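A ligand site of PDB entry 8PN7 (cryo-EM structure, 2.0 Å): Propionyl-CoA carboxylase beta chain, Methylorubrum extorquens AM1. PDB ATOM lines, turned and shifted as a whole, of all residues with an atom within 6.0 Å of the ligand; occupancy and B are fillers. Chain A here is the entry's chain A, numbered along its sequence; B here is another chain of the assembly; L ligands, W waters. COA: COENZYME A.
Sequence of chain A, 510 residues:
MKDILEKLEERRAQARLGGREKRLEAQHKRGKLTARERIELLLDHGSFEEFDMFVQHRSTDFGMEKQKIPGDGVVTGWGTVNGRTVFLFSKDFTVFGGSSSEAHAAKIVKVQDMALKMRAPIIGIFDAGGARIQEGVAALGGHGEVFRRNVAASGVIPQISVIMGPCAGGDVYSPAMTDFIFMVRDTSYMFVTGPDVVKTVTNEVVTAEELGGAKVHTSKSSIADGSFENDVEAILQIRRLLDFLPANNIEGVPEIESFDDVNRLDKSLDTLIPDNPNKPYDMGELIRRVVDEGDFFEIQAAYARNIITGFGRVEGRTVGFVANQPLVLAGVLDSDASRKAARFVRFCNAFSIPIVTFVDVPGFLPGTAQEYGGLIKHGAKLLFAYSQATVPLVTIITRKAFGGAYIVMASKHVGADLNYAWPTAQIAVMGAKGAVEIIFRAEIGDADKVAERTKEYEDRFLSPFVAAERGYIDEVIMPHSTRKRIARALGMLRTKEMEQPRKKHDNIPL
N of Cys 167 is in hydrogen-bond range of O of Tyr 189, at 2.9 Å.
The side-chain hydroxyl (OG) of Ser 99 is in hydrogen-bond range of the guanidinium group (NE) of Arg 132.
O of Gly 97 lies within hydrogen-bond range of N of Gly 129 (3.1 Å).
The side-chain hydroxyl of Ser 99 sits at hydrogen-bond distance from the backbone carbonyl oxygen of Phe 96 (2.9 Å).
O of Pro 166 is in hydrogen-bond range of N of Ala 128 (3.0 Å).
The guanidinium group (NH1) of Arg 441 of chain B lies within hydrogen-bond range of the backbone carbonyl oxygen (O) of Ile 438 of chain B (3.1 Å).
Phe 96 touches the ligand.
Ser 99 touches the ligand.
O of Ala 128 touches CDP of the ligand, 3.8 Å away.
O of Gly 129 touches C7P of the ligand, at 3.3 Å.
Arg 132 touches the ligand (CA to N1A, 3.4 Å).
OE1 of Gln 134 touches C2A of the ligand, 3.6 Å away.
Pro 166 touches the ligand (CB to CDP, 3.7 Å).
CB of Ala 168 touches O9P of the ligand, at 3.95 Å.
Asp 196 touches the ligand.
CD1 of Ile 438 of chain B touches C5P of the ligand, 3.5 Å away.
Within 4 Å of the ligand: Arg 23, Phe 96, Gly 97, Ser 99, Ala 128, Gly 129, Ala 131, Arg 132, Ile 133, Gln 134, Pro 166, Ala 168, Tyr 189, Asp 196, Ile 438 of chain B and Arg 441 of chain B.
A nitrogen (N1A) of the ligand is in hydrogen-bond range of the backbone NH (N) of Ile 133.
An oxygen (O4B) of the ligand lies close to the backbone NH (N) of Gly 97, at 3.4 Å.
The backbone carbonyl oxygen (O) of Ala 131 is in hydrogen-bond range of a nitrogen (N6A) of the ligand (2.6 Å).
The side-chain hydroxyl (OH) of Tyr 189 is in hydrogen-bond range of an oxygen (O6A) of the ligand (3.2 Å).
An oxygen (O8A) of the ligand is in salt-bridge range of the guanidinium group (NH2) of Arg 441 of chain B (3.2 Å).
The guanidinium group (NH1) of Arg 23 lies within salt-bridge range of an oxygen (O9A) of the ligand (3.4 Å).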
ATOM      1  N   ARG A  23      -5.795  -4.048  -0.925  1.00  0.00           N
ATOM      2  CA  ARG A  23      -4.701  -4.861  -1.452  1.00  0.00           C
ATOM      3  C   ARG A  23      -3.364  -4.473  -0.826  1.00  0.00           C
ATOM      4  O   ARG A  23      -2.522  -5.331  -0.563  1.00  0.00           O
ATOM      5  CB  ARG A  23      -4.645  -4.753  -2.977  1.00  0.00           C
ATOM      6  CG  ARG A  23      -5.758  -5.496  -3.681  1.00  0.00           C
ATOM      7  CD  ARG A  23      -5.583  -5.488  -5.186  1.00  0.00           C
ATOM      8  NE  ARG A  23      -6.724  -6.080  -5.878  1.00  0.00           N
ATOM      9  CZ  ARG A  23      -6.834  -7.368  -6.173  1.00  0.00           C
ATOM     10  NH1 ARG A  23      -5.893  -8.236  -5.845  1.00  0.00           N
ATOM     11  NH2 ARG A  23      -7.917  -7.799  -6.810  1.00  0.00           N
ATOM     12  N   PHE A  93       2.713  -5.566  -6.865  1.00  0.00           N
ATOM     13  CA  PHE A  93       1.934  -6.794  -6.823  1.00  0.00           C
ATOM     14  C   PHE A  93       0.439  -6.532  -6.702  1.00  0.00           C
ATOM     15  O   PHE A  93      -0.359  -7.412  -7.052  1.00  0.00           O
ATOM     16  CB  PHE A  93       2.405  -7.662  -5.652  1.00  0.00           C
ATOM     17  CG  PHE A  93       1.720  -8.990  -5.564  1.00  0.00           C
ATOM     18  CD1 PHE A  93       2.084 -10.032  -6.390  1.00  0.00           C
ATOM     19  CD2 PHE A  93       0.706  -9.201  -4.648  1.00  0.00           C
ATOM     20  CE1 PHE A  93       1.450 -11.259  -6.317  1.00  0.00           C
ATOM     21  CE2 PHE A  93       0.063 -10.424  -4.565  1.00  0.00           C
ATOM     22  CZ  PHE A  93       0.446 -11.456  -5.398  1.00  0.00           C
ATOM     23  N   PHE A  96      -2.989  -5.906 -10.815  1.00  0.00           N
ATOM     24  CA  PHE A  96      -3.078  -7.077 -11.689  1.00  0.00           C
ATOM     25  C   PHE A  96      -2.065  -8.154 -11.299  1.00  0.00           C
ATOM     26  O   PHE A  96      -1.581  -8.898 -12.150  1.00  0.00           O
ATOM     27  CB  PHE A  96      -2.911  -6.687 -13.160  1.00  0.00           C
ATOM     28  CG  PHE A  96      -3.890  -5.658 -13.629  1.00  0.00           C
ATOM     29  CD1 PHE A  96      -5.246  -5.940 -13.706  1.00  0.00           C
ATOM     30  CD2 PHE A  96      -3.460  -4.395 -14.013  1.00  0.00           C
ATOM     31  CE1 PHE A  96      -6.143  -4.990 -14.128  1.00  0.00           C
ATOM     32  CE2 PHE A  96      -4.359  -3.441 -14.448  1.00  0.00           C
ATOM     33  CZ  PHE A  96      -5.702  -3.734 -14.508  1.00  0.00           C
ATOM     34  N   GLY A  97      -1.748  -8.240 -10.014  1.00  0.00           N
ATOM     35  CA  GLY A  97      -0.766  -9.197  -9.562  1.00  0.00           C
ATOM     36  C   GLY A  97       0.645  -8.917 -10.015  1.00  0.00           C
ATOM     37  O   GLY A  97       1.472  -9.824 -10.055  1.00  0.00           O
ATOM     38  N   GLY A  98       0.950  -7.660 -10.361  1.00  0.00           N
ATOM     39  CA  GLY A  98       2.269  -7.320 -10.872  1.00  0.00           C
ATOM     40  C   GLY A  98       2.557  -7.799 -12.271  1.00  0.00           C
ATOM     41  O   GLY A  98       3.693  -7.671 -12.730  1.00  0.00           O
ATOM     42  N   SER A  99       1.552  -8.311 -12.973  1.00  0.00           N
ATOM     43  CA  SER A  99       1.778  -8.909 -14.280  1.00  0.00           C
ATOM     44  C   SER A  99       2.267  -7.877 -15.285  1.00  0.00           C
ATOM     45  O   SER A  99       1.953  -6.684 -15.196  1.00  0.00           O
ATOM     46  CB  SER A  99       0.502  -9.572 -14.795  1.00  0.00           C
ATOM     47  OG  SER A  99      -0.570  -8.643 -14.848  1.00  0.00           O
ATOM     48  N   ALA A 128       5.533 -10.132  -8.731  1.00  0.00           N
ATOM     49  CA  ALA A 128       4.703 -10.081  -9.938  1.00  0.00           C
ATOM     50  C   ALA A 128       4.155 -11.469 -10.230  1.00  0.00           C
ATOM     51  O   ALA A 128       4.261 -12.391  -9.419  1.00  0.00           O
ATOM     52  CB  ALA A 128       5.502  -9.522 -11.114  1.00  0.00           C
ATOM     53  N   GLY A 129       3.562 -11.626 -11.414  1.00  0.00           N
ATOM     54  CA  GLY A 129       2.989 -12.884 -11.843  1.00  0.00           C
ATOM     55  C   GLY A 129       3.476 -13.372 -13.198  1.00  0.00           C
ATOM     56  O   GLY A 129       3.336 -14.550 -13.516  1.00  0.00           O
ATOM     57  N   GLY A 130       4.050 -12.477 -13.988  1.00  0.00           N
ATOM     58  CA  GLY A 130       4.530 -12.803 -15.317  1.00  0.00           C
ATOM     59  C   GLY A 130       3.831 -11.965 -16.381  1.00  0.00           C
ATOM     60  O   GLY A 130       3.526 -10.791 -16.158  1.00  0.00           O
ATOM     61  N   ALA A 131       3.603 -12.574 -17.537  1.00  0.00           N
ATOM     62  CA  ALA A 131       2.901 -11.898 -18.627  1.00  0.00           C
ATOM     63  C   ALA A 131       1.420 -11.818 -18.317  1.00  0.00           C
ATOM     64  O   ALA A 131       0.811 -12.782 -17.841  1.00  0.00           O
ATOM     65  CB  ALA A 131       3.134 -12.638 -19.948  1.00  0.00           C
ATOM     66  N   ARG A 132       0.822 -10.658 -18.585  1.00  0.00           N
ATOM     67  CA  ARG A 132      -0.602 -10.464 -18.331  1.00  0.00           C
ATOM     68  C   ARG A 132      -1.411 -11.241 -19.364  1.00  0.00           C
ATOM     69  O   ARG A 132      -1.281 -11.017 -20.560  1.00  0.00           O
ATOM     70  CB  ARG A 132      -0.949  -8.981 -18.374  1.00  0.00           C
ATOM     71  CG  ARG A 132      -2.327  -8.643 -17.837  1.00  0.00           C
ATOM     72  CD  ARG A 132      -2.514  -7.146 -17.720  1.00  0.00           C
ATOM     73  NE  ARG A 132      -1.533  -6.532 -16.842  1.00  0.00           N
ATOM     74  CZ  ARG A 132      -1.423  -5.228 -16.624  1.00  0.00           C
ATOM     75  NH1 ARG A 132      -2.227  -4.362 -17.226  1.00  0.00           N
ATOM     76  NH2 ARG A 132      -0.490  -4.775 -15.803  1.00  0.00           N
ATOM     77  N   ILE A 133      -2.253 -12.161 -18.878  1.00  0.00           N
ATOM     78  CA  ILE A 133      -2.923 -13.105 -19.766  1.00  0.00           C
ATOM     79  C   ILE A 133      -3.926 -12.390 -20.667  1.00  0.00           C
ATOM     80  O   ILE A 133      -4.110 -12.759 -21.831  1.00  0.00           O
ATOM     81  CB  ILE A 133      -3.590 -14.220 -18.939  1.00  0.00           C
ATOM     82  CG1 ILE A 133      -4.372 -15.177 -19.843  1.00  0.00           C
ATOM     83  CG2 ILE A 133      -4.489 -13.645 -17.856  1.00  0.00           C
ATOM     84  CD1 ILE A 133      -3.515 -15.901 -20.853  1.00  0.00           C
ATOM     85  N   GLN A 134      -4.591 -11.357 -20.151  1.00  0.00           N
ATOM     86  CA  GLN A 134      -5.636 -10.676 -20.916  1.00  0.00           C
ATOM     87  C   GLN A 134      -5.096  -9.947 -22.138  1.00  0.00           C
ATOM     88  O   GLN A 134      -5.854  -9.696 -23.072  1.00  0.00           O
ATOM     89  CB  GLN A 134      -6.393  -9.698 -20.030  1.00  0.00           C
ATOM     90  CG  GLN A 134      -7.293 -10.338 -18.983  1.00  0.00           C
ATOM     91  CD  GLN A 134      -6.536 -10.746 -17.724  1.00  0.00           C
ATOM     92  OE1 GLN A 134      -5.335 -10.483 -17.600  1.00  0.00           O
ATOM     93  NE2 GLN A 134      -7.229 -11.390 -16.797  1.00  0.00           N
ATOM     94  N   PRO A 166       6.252 -13.468  -5.638  1.00  0.00           N
ATOM     95  CA  PRO A 166       6.179 -14.468  -6.709  1.00  0.00           C
ATOM     96  C   PRO A 166       6.881 -13.989  -7.969  1.00  0.00           C
ATOM     97  O   PRO A 166       6.869 -12.797  -8.296  1.00  0.00           O
ATOM     98  CB  PRO A 166       4.666 -14.638  -6.946  1.00  0.00           C
ATOM     99  CG  PRO A 166       4.040 -14.188  -5.671  1.00  0.00           C
ATOM    100  CD  PRO A 166       4.919 -13.101  -5.143  1.00  0.00           C
ATOM    101  N   CYS A 167       7.506 -14.922  -8.673  1.00  0.00           N
ATOM    102  CA  CYS A 167       8.159 -14.667  -9.956  1.00  0.00           C
ATOM    103  C   CYS A 167       7.991 -15.936 -10.782  1.00  0.00           C
ATOM    104  O   CYS A 167       8.713 -16.915 -10.567  1.00  0.00           O
ATOM    105  CB  CYS A 167       9.621 -14.287  -9.784  1.00  0.00           C
ATOM    106  SG  CYS A 167      10.427 -13.668 -11.278  1.00  0.00           S
ATOM    107  N   ALA A 168       7.038 -15.930 -11.702  1.00  0.00           N
ATOM    108  CA  ALA A 168       6.639 -17.135 -12.415  1.00  0.00           C
ATOM    109  C   ALA A 168       6.558 -16.878 -13.906  1.00  0.00           C
ATOM    110  O   ALA A 168       6.413 -15.747 -14.359  1.00  0.00           O
ATOM    111  CB  ALA A 168       5.291 -17.661 -11.903  1.00  0.00           C
ATOM    112  N   TYR A 189       9.467 -16.649  -4.479  1.00  0.00           N
ATOM    113  CA  TYR A 189       9.781 -17.892  -5.156  1.00  0.00           C
ATOM    114  C   TYR A 189       9.892 -17.636  -6.653  1.00  0.00           C
ATOM    115  O   TYR A 189       9.323 -16.682  -7.187  1.00  0.00           O
ATOM    116  CB  TYR A 189       8.732 -18.978  -4.870  1.00  0.00           C
ATOM    117  CG  TYR A 189       7.292 -18.525  -4.938  1.00  0.00           C
ATOM    118  CD1 TYR A 189       6.623 -18.469  -6.152  1.00  0.00           C
ATOM    119  CD2 TYR A 189       6.606 -18.163  -3.793  1.00  0.00           C
ATOM    120  CE1 TYR A 189       5.307 -18.057  -6.220  1.00  0.00           C
ATOM    121  CE2 TYR A 189       5.292 -17.755  -3.848  1.00  0.00           C
ATOM    122  CZ  TYR A 189       4.643 -17.706  -5.059  1.00  0.00           C
ATOM    123  OH  TYR A 189       3.338 -17.303  -5.125  1.00  0.00           O
ATOM    124  N   PHE A 191       9.974 -19.863 -10.475  1.00  0.00           N
ATOM    125  CA  PHE A 191       9.926 -21.061 -11.281  1.00  0.00           C
ATOM    126  C   PHE A 191       9.390 -20.722 -12.660  1.00  0.00           C
ATOM    127  O   PHE A 191       8.577 -19.806 -12.821  1.00  0.00           O
ATOM    128  CB  PHE A 191       9.074 -22.170 -10.634  1.00  0.00           C
ATOM    129  CG  PHE A 191       7.851 -21.669  -9.915  1.00  0.00           C
ATOM    130  CD1 PHE A 191       6.792 -21.114 -10.610  1.00  0.00           C
ATOM    131  CD2 PHE A 191       7.766 -21.756  -8.535  1.00  0.00           C
ATOM    132  CE1 PHE A 191       5.677 -20.661  -9.943  1.00  0.00           C
ATOM    133  CE2 PHE A 191       6.651 -21.304  -7.868  1.00  0.00           C
ATOM    134  CZ  PHE A 191       5.602 -20.761  -8.569  1.00  0.00           C
ATOM    135  N   GLY A 194       4.461 -23.252 -12.854  1.00  0.00           N
ATOM    136  CA  GLY A 194       3.877 -23.228 -11.534  1.00  0.00           C
ATOM    137  C   GLY A 194       3.476 -24.591 -11.043  1.00  0.00           C
ATOM    138  O   GLY A 194       3.475 -25.596 -11.776  1.00  0.00           O
ATOM    139  N   PRO A 195       3.116 -24.657  -9.752  1.00  0.00           N
ATOM    140  CA  PRO A 195       2.755 -25.956  -9.150  1.00  0.00           C
ATOM    141  C   PRO A 195       1.554 -26.631  -9.792  1.00  0.00           C
ATOM    142  O   PRO A 195       1.505 -27.872  -9.821  1.00  0.00           O
ATOM    143  CB  PRO A 195       2.471 -25.586  -7.681  1.00  0.00           C
ATOM    144  CG  PRO A 195       3.219 -24.318  -7.468  1.00  0.00           C
ATOM    145  CD  PRO A 195       3.142 -23.572  -8.768  1.00  0.00           C
ATOM    146  N   ASP A 196       0.570 -25.873 -10.274  1.00  0.00           N
ATOM    147  CA  ASP A 196      -0.626 -26.479 -10.850  1.00  0.00           C
ATOM    148  C   ASP A 196      -0.302 -27.271 -12.117  1.00  0.00           C
ATOM    149  O   ASP A 196      -0.737 -28.414 -12.278  1.00  0.00           O
ATOM    150  CB  ASP A 196      -1.675 -25.406 -11.132  1.00  0.00           C
ATOM    151  CG  ASP A 196      -1.107 -24.233 -11.912  1.00  0.00           C
ATOM    152  OD1 ASP A 196       0.070 -23.874 -11.690  1.00  0.00           O
ATOM    153  OD2 ASP A 196      -1.841 -23.665 -12.747  1.00  0.00           O
ATOM    154  N   ALA A 208       4.477 -23.833  -3.703  1.00  0.00           N
ATOM    155  CA  ALA A 208       5.347 -22.838  -4.334  1.00  0.00           C
ATOM    156  C   ALA A 208       6.701 -22.784  -3.655  1.00  0.00           C
ATOM    157  O   ALA A 208       7.740 -22.654  -4.323  1.00  0.00           O
ATOM    158  CB  ALA A 208       4.671 -21.469  -4.320  1.00  0.00           C
ATOM    159  N   MET B 430      -0.640 -19.012 -24.005  1.00  0.00           N
ATOM    160  CA  MET B 430      -0.766 -20.399 -23.583  1.00  0.00           C
ATOM    161  C   MET B 430      -1.916 -21.030 -24.367  1.00  0.00           C
ATOM    162  O   MET B 430      -2.517 -20.410 -25.243  1.00  0.00           O
ATOM    163  CB  MET B 430      -0.986 -20.504 -22.078  1.00  0.00           C
ATOM    164  CG  MET B 430      -2.258 -19.825 -21.588  1.00  0.00           C
ATOM    165  SD  MET B 430      -2.557 -20.099 -19.825  1.00  0.00           S
ATOM    166  CE  MET B 430      -1.067 -19.399 -19.120  1.00  0.00           C
ATOM    167  N   ILE B 438      -7.854 -19.160 -16.515  1.00  0.00           N
ATOM    168  CA  ILE B 438      -7.296 -18.038 -15.782  1.00  0.00           C
ATOM    169  C   ILE B 438      -8.168 -16.785 -15.938  1.00  0.00           C
ATOM    170  O   ILE B 438      -8.452 -16.096 -14.961  1.00  0.00           O
ATOM    171  CB  ILE B 438      -5.852 -17.783 -16.225  1.00  0.00           C
ATOM    172  CG1 ILE B 438      -4.969 -18.977 -15.874  1.00  0.00           C
ATOM    173  CG2 ILE B 438      -5.312 -16.512 -15.572  1.00  0.00           C
ATOM    174  CD1 ILE B 438      -3.554 -18.859 -16.376  1.00  0.00           C
ATOM    175  N   ARG B 441     -11.826 -17.371 -14.302  1.00  0.00           N
ATOM    176  CA  ARG B 441     -11.718 -18.176 -13.098  1.00  0.00           C
ATOM    177  C   ARG B 441     -12.988 -18.114 -12.250  1.00  0.00           C
ATOM    178  O   ARG B 441     -13.283 -19.055 -11.506  1.00  0.00           O
ATOM    179  CB  ARG B 441     -10.511 -17.719 -12.269  1.00  0.00           C
ATOM    180  CG  ARG B 441     -10.521 -16.228 -11.948  1.00  0.00           C
ATOM    181  CD  ARG B 441      -9.217 -15.783 -11.316  1.00  0.00           C
ATOM    182  NE  ARG B 441      -9.224 -14.350 -10.998  1.00  0.00           N
ATOM    183  CZ  ARG B 441      -8.862 -13.398 -11.845  1.00  0.00           C
ATOM    184  NH1 ARG B 441      -8.442 -13.685 -13.064  1.00  0.00           N
ATOM    185  NH2 ARG B 441      -8.909 -12.131 -11.444  1.00  0.00           N
HETATM  186  N1A COA L   1      -1.777 -12.285 -15.772  1.00  0.00           N
HETATM  187  C2A COA L   1      -2.868 -11.679 -15.316  1.00  0.00           C
HETATM  188  N3A COA L   1      -3.213 -11.695 -14.043  1.00  0.00           N
HETATM  189  C4A COA L   1      -2.468 -12.324 -13.153  1.00  0.00           C
HETATM  190  C5A COA L   1      -1.272 -12.995 -13.606  1.00  0.00           C
HETATM  191  C6A COA L   1      -0.979 -12.943 -14.951  1.00  0.00           C
HETATM  192  N6A COA L   1       0.208 -13.602 -15.467  1.00  0.00           N
HETATM  193  N7A COA L   1      -0.683 -13.595 -12.410  1.00  0.00           N
HETATM  194  C8A COA L   1      -1.471 -13.282 -11.377  1.00  0.00           C
HETATM  195  N9A COA L   1      -2.481 -12.560 -11.836  1.00  0.00           N
HETATM  196  C1B COA L   1      -3.507 -12.062 -10.996  1.00  0.00           C
HETATM  197  C2B COA L   1      -4.378 -13.163 -10.501  1.00  0.00           C
HETATM  198  O2B COA L   1      -5.479 -13.369 -11.418  1.00  0.00           O
HETATM  199  C3B COA L   1      -4.882 -12.705  -9.219  1.00  0.00           C
HETATM  200  O3B COA L   1      -6.088 -11.932  -9.449  1.00  0.00           O
HETATM  201  P3B COA L   1      -7.197 -11.806  -8.239  1.00  0.00           P
HETATM  202  O7A COA L   1      -7.879 -13.060  -7.929  1.00  0.00           O
HETATM  203  O8A COA L   1      -8.278 -10.873  -8.521  1.00  0.00           O
HETATM  204  O9A COA L   1      -6.651 -11.357  -6.969  1.00  0.00           O
HETATM  205  C4B COA L   1      -3.836 -11.803  -8.652  1.00  0.00           C
HETATM  206  O4B COA L   1      -2.917 -11.424  -9.765  1.00  0.00           O
HETATM  207  C5B COA L   1      -3.093 -12.518  -7.579  1.00  0.00           C
HETATM  208  O5B COA L   1      -2.643 -13.761  -8.052  1.00  0.00           O
HETATM  209  P1A COA L   1      -3.260 -15.145  -7.358  1.00  0.00           P
HETATM  210  O1A COA L   1      -4.421 -15.632  -8.082  1.00  0.00           O
HETATM  211  O2A COA L   1      -3.831 -14.866  -6.053  1.00  0.00           O
HETATM  212  O3A COA L   1      -2.077 -16.313  -7.266  1.00  0.00           O
HETATM  213  P2A COA L   1      -0.986 -16.422  -6.016  1.00  0.00           P
HETATM  214  O4A COA L   1      -1.086 -15.267  -5.127  1.00  0.00           O
HETATM  215  O5A COA L   1      -1.320 -17.519  -5.105  1.00  0.00           O
HETATM  216  O6A COA L   1       0.554 -16.595  -6.623  1.00  0.00           O
HETATM  217  CBP COA L   1       1.516 -16.596  -8.869  1.00  0.00           C
HETATM  218  CCP COA L   1       0.964 -15.731  -7.690  1.00  0.00           C
HETATM  219  CDP COA L   1       2.424 -15.726  -9.745  1.00  0.00           C
HETATM  220  CEP COA L   1       2.333 -17.767  -8.308  1.00  0.00           C
HETATM  221  CAP COA L   1       0.335 -17.154  -9.702  1.00  0.00           C
HETATM  222  OAP COA L   1      -0.724 -16.266  -9.665  1.00  0.00           O
HETATM  223  C9P COA L   1       0.753 -17.384 -11.157  1.00  0.00           C
HETATM  224  O9P COA L   1       1.419 -18.322 -11.451  1.00  0.00           O
HETATM  225  N8P COA L   1       0.322 -16.439 -12.213  1.00  0.00           N
HETATM  226  C7P COA L   1       0.725 -16.642 -13.612  1.00  0.00           C
HETATM  227  C6P COA L   1      -0.529 -16.994 -14.447  1.00  0.00           C
HETATM  228  C5P COA L   1      -1.084 -18.362 -13.973  1.00  0.00           C
HETATM  229  O5P COA L   1      -0.632 -19.367 -14.405  1.00  0.00           O
HETATM  230  N4P COA L   1      -2.179 -18.407 -12.981  1.00  0.00           N
HETATM  231  C3P COA L   1      -2.711 -19.693 -12.530  1.00  0.00           C
HETATM  232  C2P COA L   1      -1.740 -20.341 -11.536  1.00  0.00           C
HETATM  233  S1P COA L   1      -2.323 -20.075  -9.846  1.00  0.00           S
HETATM  234  O   HOH W   1       1.281 -20.867  -9.667  1.00  0.00           O
HETATM  235  O   HOH W   2      -5.849  -8.819 -10.145  1.00  0.00           O
HETATM  236  O   HOH W   3      -1.948 -13.299  -3.149  1.00  0.00           O
